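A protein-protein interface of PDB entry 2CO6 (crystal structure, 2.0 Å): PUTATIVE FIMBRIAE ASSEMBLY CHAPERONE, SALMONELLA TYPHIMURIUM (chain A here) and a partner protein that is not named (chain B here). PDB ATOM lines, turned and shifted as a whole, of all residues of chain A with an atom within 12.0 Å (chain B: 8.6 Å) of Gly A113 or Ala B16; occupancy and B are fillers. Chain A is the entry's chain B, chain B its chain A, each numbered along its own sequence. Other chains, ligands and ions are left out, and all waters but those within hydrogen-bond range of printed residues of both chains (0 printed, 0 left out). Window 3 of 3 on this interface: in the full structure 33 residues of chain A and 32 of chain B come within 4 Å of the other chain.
The backbone NH (N) of Thr A115 is in hydrogen-bond range of the backbone carbonyl oxygen (O) of Asp B112 (2.9 Å). The side-chain hydroxyl (OG1) of Thr B113 lies within hydrogen-bond range of the side-chain hydroxyl (OG1) of Thr A115 (3.0 Å). The backbone NH (N) of Tyr B114 is in hydrogen-bond range of the backbone carbonyl oxygen (O) of Thr A115, 2.7 Å away. The backbone carbonyl oxygen (O) of Tyr B114 lies within hydrogen-bond range of the backbone NH (N) of Asp A117 (3.0 Å).
The backbone carbonyl oxygen (O) of Gly B13 lies within hydrogen-bond range of the side-chain amino group (NZ) of Lys B15, at 2.8 Å. The backbone carbonyl oxygen (O) of Lys B15 sits at hydrogen-bond distance from the side-chain amide nitrogen (ND2) of Asn B19. The backbone NH of Gly B17 sits at hydrogen-bond distance from the backbone carbonyl oxygen of Val B109 (2.7 Å). N of Asn B61 sits at hydrogen-bond distance from OD2 of Asp B112 (2.9 Å). The backbone carbonyl oxygen (O) of Thr B110 sits at hydrogen-bond distance from the side-chain hydroxyl (OH) of Tyr B114 (2.5 Å). N of Leu A116 sits at hydrogen-bond distance from OG of Ser A7 (2.8 Å).
Gly A113 touches Ala B16. Gly A113 touches Ala B111 (O to CB, 3.6 Å). Asp B112 touches Gly A113. Lys B15 touches Ala A114 (C to CB, 3.8 Å). N of Ala B16 touches CB of Ala A114 (3.8 Å). CB of Ala A114 touches CG1 of Val B109, at 3.9 Å. O of Asp B112 touches CA of Ala A114, 3.5 Å away. Leu A116 touches Leu B14 (CD2 to CD2, 3.5 Å). Tyr B114 touches Leu A116. Thr B113 touches Asp A117.
Gly A113 touches just these residues of chain B: Ala B16, Ala B111 and Asp B112. Of the printed residues of chain B, Leu A116 touches Leu B14 and Tyr B114. Of the printed residues of chain B, Asp A117 touches Thr B113 (3.7 Å) and Tyr B114 (3.0 Å). Leu B14 touches two residues of chain A. Of chain A, only Ala A114 comes within 4 Å of Lys B15. Ala B16 touches just these residues of chain A: Gly A113 and Ala A114. No residue of chain A comes within 4 Å of Gly B17. No residue of chain A comes within 4 Å of Asn B108. No residue of chain A comes within 4 Å of Thr B110. Of chain A, only Gly A113 (3.6 Å) comes within 4 Å of Ala B111. Printed residues of chain A within 4 Å of Thr B113: Thr A115 and Asp A117. The nearest printed residue of chain B that does not touch Gly A113 is Lys B15 (5.4 Å).
Of the 17 printed residues of chain B, 8 touch a printed residue of chain A. Hydrophobic or aromatic side chains of chain B within 4 Å of the printed part of chain A: Leu B14, Ala B16, Val B109, Ala B111 and Tyr B114. Among the printed residues, 15 pairs touch across the chains. Among the printed residues, no Asp or Glu carboxylate lies within 4 Å of a Lys or Arg side-chain nitrogen of the other chain.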
ATOM      1  N   LEU A   5     -16.798 -14.330  -1.453  1.00  0.00           N
ATOM      2  CA  LEU A   5     -15.620 -15.265  -1.412  1.00  0.00           C
ATOM      3  C   LEU A   5     -15.830 -16.595  -2.182  1.00  0.00           C
ATOM      4  O   LEU A   5     -16.872 -17.253  -2.046  1.00  0.00           O
ATOM      5  CB  LEU A   5     -15.165 -15.514   0.031  1.00  0.00           C
ATOM      6  CG  LEU A   5     -13.758 -16.114   0.217  1.00  0.00           C
ATOM      7  CD1 LEU A   5     -12.865 -15.235   1.095  1.00  0.00           C
ATOM      8  CD2 LEU A   5     -13.828 -17.526   0.771  1.00  0.00           C
ATOM      9  N   ASN A   6     -14.801 -16.964  -2.959  1.00  0.00           N
ATOM     10  CA  ASN A   6     -14.841 -17.998  -3.994  1.00  0.00           C
ATOM     11  C   ASN A   6     -15.242 -19.386  -3.541  1.00  0.00           C
ATOM     12  O   ASN A   6     -16.126 -20.011  -4.134  1.00  0.00           O
ATOM     13  CB  ASN A   6     -13.463 -18.122  -4.642  1.00  0.00           C
ATOM     14  CG  ASN A   6     -12.730 -16.794  -4.739  1.00  0.00           C
ATOM     15  OD1 ASN A   6     -12.221 -16.259  -3.730  1.00  0.00           O
ATOM     16  ND2 ASN A   6     -12.631 -16.272  -5.965  1.00  0.00           N
ATOM     17  N   SER A   7     -14.546 -19.881  -2.521  1.00  0.00           N
ATOM     18  CA  SER A   7     -14.735 -21.237  -2.035  1.00  0.00           C
ATOM     19  C   SER A   7     -15.810 -21.237  -0.964  1.00  0.00           C
ATOM     20  O   SER A   7     -15.860 -20.320  -0.131  1.00  0.00           O
ATOM     21  CB  SER A   7     -13.425 -21.777  -1.449  1.00  0.00           C
ATOM     22  OG  SER A   7     -12.346 -21.571  -2.344  1.00  0.00           O
ATOM     23  N   GLY A 113      -9.267 -16.825 -10.466  1.00  0.00           N
ATOM     24  CA  GLY A 113      -8.039 -17.190  -9.739  1.00  0.00           C
ATOM     25  C   GLY A 113      -8.085 -18.642  -9.295  1.00  0.00           C
ATOM     26  O   GLY A 113      -8.645 -19.498  -9.994  1.00  0.00           O
ATOM     27  N   ALA A 114      -7.520 -18.915  -8.121  1.00  0.00           N
ATOM     28  CA  ALA A 114      -7.424 -20.282  -7.595  1.00  0.00           C
ATOM     29  C   ALA A 114      -8.484 -20.520  -6.540  1.00  0.00           C
ATOM     30  O   ALA A 114      -8.521 -19.795  -5.542  1.00  0.00           O
ATOM     31  CB  ALA A 114      -6.052 -20.514  -6.993  1.00  0.00           C
ATOM     32  N   THR A 115      -9.344 -21.523  -6.737  1.00  0.00           N
ATOM     33  CA  THR A 115     -10.379 -21.775  -5.747  1.00  0.00           C
ATOM     34  C   THR A 115     -10.286 -23.198  -5.139  1.00  0.00           C
ATOM     35  O   THR A 115      -9.691 -24.089  -5.735  1.00  0.00           O
ATOM     36  CB  THR A 115     -11.790 -21.456  -6.303  1.00  0.00           C
ATOM     37  OG1 THR A 115     -12.149 -22.411  -7.289  1.00  0.00           O
ATOM     38  CG2 THR A 115     -11.826 -20.115  -6.975  1.00  0.00           C
ATOM     39  N   LEU A 116     -10.843 -23.381  -3.939  1.00  0.00           N
ATOM     40  CA  LEU A 116     -10.907 -24.690  -3.305  1.00  0.00           C
ATOM     41  C   LEU A 116     -12.312 -25.253  -3.349  1.00  0.00           C
ATOM     42  O   LEU A 116     -13.304 -24.513  -3.229  1.00  0.00           O
ATOM     43  CB  LEU A 116     -10.445 -24.610  -1.855  1.00  0.00           C
ATOM     44  CG  LEU A 116      -9.074 -24.007  -1.533  1.00  0.00           C
ATOM     45  CD1 LEU A 116      -8.950 -23.774  -0.017  1.00  0.00           C
ATOM     46  CD2 LEU A 116      -7.940 -24.883  -2.015  1.00  0.00           C
ATOM     47  N   ASP A 117     -12.393 -26.568  -3.532  1.00  0.00           N
ATOM     48  CA  ASP A 117     -13.645 -27.312  -3.434  1.00  0.00           C
ATOM     49  C   ASP A 117     -13.440 -28.219  -2.212  1.00  0.00           C
ATOM     50  O   ASP A 117     -12.760 -29.258  -2.254  1.00  0.00           O
ATOM     51  CB  ASP A 117     -13.925 -28.072  -4.739  1.00  0.00           C
ATOM     52  CG  ASP A 117     -15.056 -29.094  -4.612  1.00  0.00           C
ATOM     53  OD1 ASP A 117     -16.027 -28.861  -3.865  1.00  0.00           O
ATOM     54  OD2 ASP A 117     -14.987 -30.141  -5.296  1.00  0.00           O
ATOM     55  N   GLY B  13      -6.463 -15.730   0.948  1.00  0.00           N
ATOM     56  CA  GLY B  13      -5.014 -15.790   0.784  1.00  0.00           C
ATOM     57  C   GLY B  13      -4.626 -16.453  -0.515  1.00  0.00           C
ATOM     58  O   GLY B  13      -3.925 -15.861  -1.323  1.00  0.00           O
ATOM     59  N   LEU B  14      -5.106 -17.678  -0.716  1.00  0.00           N
ATOM     60  CA  LEU B  14      -4.885 -18.413  -1.945  1.00  0.00           C
ATOM     61  C   LEU B  14      -5.159 -17.568  -3.182  1.00  0.00           C
ATOM     62  O   LEU B  14      -6.220 -16.965  -3.323  1.00  0.00           O
ATOM     63  CB  LEU B  14      -5.765 -19.683  -1.963  1.00  0.00           C
ATOM     64  CG  LEU B  14      -5.522 -20.714  -3.064  1.00  0.00           C
ATOM     65  CD1 LEU B  14      -4.100 -21.288  -3.055  1.00  0.00           C
ATOM     66  CD2 LEU B  14      -6.554 -21.816  -2.948  1.00  0.00           C
ATOM     67  N   LYS B  15      -4.177 -17.512  -4.072  1.00  0.00           N
ATOM     68  CA  LYS B  15      -4.361 -16.833  -5.336  1.00  0.00           C
ATOM     69  C   LYS B  15      -3.638 -17.587  -6.434  1.00  0.00           C
ATOM     70  O   LYS B  15      -2.714 -18.366  -6.162  1.00  0.00           O
ATOM     71  CB  LYS B  15      -3.905 -15.353  -5.252  1.00  0.00           C
ATOM     72  CG  LYS B  15      -2.582 -15.116  -4.544  1.00  0.00           C
ATOM     73  CD  LYS B  15      -2.239 -13.625  -4.560  1.00  0.00           C
ATOM     74  CE  LYS B  15      -1.662 -13.142  -3.235  1.00  0.00           C
ATOM     75  NZ  LYS B  15      -2.483 -13.573  -2.100  1.00  0.00           N
ATOM     76  N   ALA B  16      -4.083 -17.366  -7.673  1.00  0.00           N
ATOM     77  CA  ALA B  16      -3.343 -17.784  -8.856  1.00  0.00           C
ATOM     78  C   ALA B  16      -1.986 -17.051  -8.846  1.00  0.00           C
ATOM     79  O   ALA B  16      -1.902 -15.899  -8.395  1.00  0.00           O
ATOM     80  CB  ALA B  16      -4.132 -17.455 -10.083  1.00  0.00           C
ATOM     81  N   GLY B  17      -0.925 -17.730  -9.281  1.00  0.00           N
ATOM     82  CA  GLY B  17       0.404 -17.115  -9.299  1.00  0.00           C
ATOM     83  C   GLY B  17       1.131 -17.359  -7.985  1.00  0.00           C
ATOM     84  O   GLY B  17       0.753 -18.244  -7.227  1.00  0.00           O
ATOM     85  N   LYS B  18       2.171 -16.570  -7.714  1.00  0.00           N
ATOM     86  CA  LYS B  18       3.005 -16.805  -6.539  1.00  0.00           C
ATOM     87  C   LYS B  18       2.227 -16.521  -5.268  1.00  0.00           C
ATOM     88  O   LYS B  18       1.562 -15.486  -5.144  1.00  0.00           O
ATOM     89  CB  LYS B  18       4.291 -15.963  -6.571  1.00  0.00           C
ATOM     90  CG  LYS B  18       5.443 -16.529  -5.695  1.00  0.00           C
ATOM     91  CD  LYS B  18       6.144 -17.710  -6.383  1.00  0.00           C
ATOM     92  CE  LYS B  18       7.314 -18.251  -5.554  1.00  0.00           C
ATOM     93  NZ  LYS B  18       8.360 -17.199  -5.299  1.00  0.00           N
ATOM     94  N   ASN B  19       2.326 -17.466  -4.335  1.00  0.00           N
ATOM     95  CA  ASN B  19       1.704 -17.367  -3.029  1.00  0.00           C
ATOM     96  C   ASN B  19       2.733 -17.118  -1.942  1.00  0.00           C
ATOM     97  O   ASN B  19       3.925 -17.366  -2.132  1.00  0.00           O
ATOM     98  CB  ASN B  19       0.879 -18.624  -2.738  1.00  0.00           C
ATOM     99  CG  ASN B  19      -0.467 -18.588  -3.433  1.00  0.00           C
ATOM    100  OD1 ASN B  19      -1.474 -18.231  -2.829  1.00  0.00           O
ATOM    101  ND2 ASN B  19      -0.483 -18.904  -4.721  1.00  0.00           N
ATOM    102  N   ASN B  61      -9.481 -28.713 -13.676  1.00  0.00           N
ATOM    103  CA  ASN B  61      -9.434 -28.414 -15.105  1.00  0.00           C
ATOM    104  C   ASN B  61      -8.109 -28.709 -15.765  1.00  0.00           C
ATOM    105  O   ASN B  61      -8.061 -29.025 -16.947  1.00  0.00           O
ATOM    106  CB  ASN B  61      -9.824 -26.956 -15.375  1.00  0.00           C
ATOM    107  CG  ASN B  61     -11.214 -26.652 -14.918  1.00  0.00           C
ATOM    108  OD1 ASN B  61     -12.143 -27.436 -15.150  1.00  0.00           O
ATOM    109  ND2 ASN B  61     -11.372 -25.533 -14.214  1.00  0.00           N
ATOM    110  N   LEU B 102      -0.664 -24.009   2.187  1.00  0.00           N
ATOM    111  CA  LEU B 102       0.225 -24.417   1.094  1.00  0.00           C
ATOM    112  C   LEU B 102       1.581 -24.774   1.687  1.00  0.00           C
ATOM    113  O   LEU B 102       2.284 -23.901   2.211  1.00  0.00           O
ATOM    114  CB  LEU B 102       0.393 -23.298   0.068  1.00  0.00           C
ATOM    115  CG  LEU B 102      -0.843 -22.952  -0.754  1.00  0.00           C
ATOM    116  CD1 LEU B 102      -0.601 -21.663  -1.582  1.00  0.00           C
ATOM    117  CD2 LEU B 102      -1.326 -24.143  -1.652  1.00  0.00           C
ATOM    118  N   GLN B 107       4.659 -21.360  -3.354  1.00  0.00           N
ATOM    119  CA  GLN B 107       4.161 -22.123  -4.481  1.00  0.00           C
ATOM    120  C   GLN B 107       3.545 -21.213  -5.517  1.00  0.00           C
ATOM    121  O   GLN B 107       2.851 -20.240  -5.184  1.00  0.00           O
ATOM    122  CB  GLN B 107       3.110 -23.144  -4.024  1.00  0.00           C
ATOM    123  CG  GLN B 107       3.660 -24.360  -3.309  1.00  0.00           C
ATOM    124  CD  GLN B 107       2.568 -25.332  -2.895  1.00  0.00           C
ATOM    125  OE1 GLN B 107       1.807 -25.843  -3.730  1.00  0.00           O
ATOM    126  NE2 GLN B 107       2.484 -25.600  -1.600  1.00  0.00           N
ATOM    127  N   ASN B 108       3.787 -21.532  -6.783  1.00  0.00           N
ATOM    128  CA  ASN B 108       3.159 -20.820  -7.880  1.00  0.00           C
ATOM    129  C   ASN B 108       1.973 -21.622  -8.369  1.00  0.00           C
ATOM    130  O   ASN B 108       2.142 -22.704  -8.917  1.00  0.00           O
ATOM    131  CB  ASN B 108       4.157 -20.616  -9.006  1.00  0.00           C
ATOM    132  CG  ASN B 108       3.877 -19.380  -9.799  1.00  0.00           C
ATOM    133  OD1 ASN B 108       4.767 -18.543 -10.003  1.00  0.00           O
ATOM    134  ND2 ASN B 108       2.641 -19.243 -10.261  1.00  0.00           N
ATOM    135  N   VAL B 109       0.774 -21.094  -8.164  1.00  0.00           N
ATOM    136  CA  VAL B 109      -0.428 -21.908  -8.309  1.00  0.00           C
ATOM    137  C   VAL B 109      -1.164 -21.543  -9.586  1.00  0.00           C
ATOM    138  O   VAL B 109      -1.402 -20.363  -9.847  1.00  0.00           O
ATOM    139  CB  VAL B 109      -1.347 -21.754  -7.053  1.00  0.00           C
ATOM    140  CG1 VAL B 109      -2.700 -22.467  -7.235  1.00  0.00           C
ATOM    141  CG2 VAL B 109      -0.619 -22.264  -5.779  1.00  0.00           C
ATOM    142  N   THR B 110      -1.522 -22.548 -10.379  1.00  0.00           N
ATOM    143  CA  THR B 110      -2.330 -22.318 -11.575  1.00  0.00           C
ATOM    144  C   THR B 110      -3.818 -22.093 -11.270  1.00  0.00           C
ATOM    145  O   THR B 110      -4.410 -22.827 -10.470  1.00  0.00           O
ATOM    146  CB  THR B 110      -2.190 -23.484 -12.577  1.00  0.00           C
ATOM    147  OG1 THR B 110      -0.801 -23.772 -12.771  1.00  0.00           O
ATOM    148  CG2 THR B 110      -2.847 -23.145 -13.916  1.00  0.00           C
ATOM    149  N   ALA B 111      -4.421 -21.083 -11.915  1.00  0.00           N
ATOM    150  CA  ALA B 111      -5.846 -20.839 -11.799  1.00  0.00           C
ATOM    151  C   ALA B 111      -6.595 -22.107 -12.128  1.00  0.00           C
ATOM    152  O   ALA B 111      -6.619 -22.566 -13.267  1.00  0.00           O
ATOM    153  CB  ALA B 111      -6.306 -19.712 -12.707  1.00  0.00           C
ATOM    154  N   ASP B 112      -7.198 -22.675 -11.100  1.00  0.00           N
ATOM    155  CA  ASP B 112      -8.010 -23.864 -11.236  1.00  0.00           C
ATOM    156  C   ASP B 112      -8.843 -23.992  -9.952  1.00  0.00           C
ATOM    157  O   ASP B 112      -8.777 -23.133  -9.087  1.00  0.00           O
ATOM    158  CB  ASP B 112      -7.092 -25.067 -11.414  1.00  0.00           C
ATOM    159  CG  ASP B 112      -7.751 -26.219 -12.133  1.00  0.00           C
ATOM    160  OD1 ASP B 112      -6.998 -27.072 -12.636  1.00  0.00           O
ATOM    161  OD2 ASP B 112      -8.993 -26.293 -12.194  1.00  0.00           O
ATOM    162  N   THR B 113      -9.676 -25.023  -9.880  1.00  0.00           N
ATOM    163  CA  THR B 113     -10.390 -25.392  -8.657  1.00  0.00           C
ATOM    164  C   THR B 113      -9.706 -26.635  -8.097  1.00  0.00           C
ATOM    165  O   THR B 113      -9.618 -27.643  -8.784  1.00  0.00           O
ATOM    166  CB  THR B 113     -11.910 -25.686  -8.928  1.00  0.00           C
ATOM    167  OG1 THR B 113     -12.556 -24.506  -9.424  1.00  0.00           O
ATOM    168  CG2 THR B 113     -12.620 -26.110  -7.655  1.00  0.00           C
ATOM    169  N   TYR B 114      -9.215 -26.551  -6.862  1.00  0.00           N
ATOM    170  CA  TYR B 114      -8.532 -27.676  -6.203  1.00  0.00           C
ATOM    171  C   TYR B 114      -9.384 -28.344  -5.106  1.00  0.00           C
ATOM    172  O   TYR B 114      -9.681 -27.737  -4.080  1.00  0.00           O
ATOM    173  CB  TYR B 114      -7.210 -27.219  -5.613  1.00  0.00           C
ATOM    174  CG  TYR B 114      -6.282 -26.625  -6.646  1.00  0.00           C
ATOM    175  CD1 TYR B 114      -6.415 -25.288  -7.057  1.00  0.00           C
ATOM    176  CD2 TYR B 114      -5.282 -27.387  -7.211  1.00  0.00           C
ATOM    177  CE1 TYR B 114      -5.565 -24.748  -8.007  1.00  0.00           C
ATOM    178  CE2 TYR B 114      -4.435 -26.873  -8.150  1.00  0.00           C
ATOM    179  CZ  TYR B 114      -4.566 -25.550  -8.549  1.00  0.00           C
ATOM    180  OH  TYR B 114      -3.706 -25.068  -9.502  1.00  0.00           O
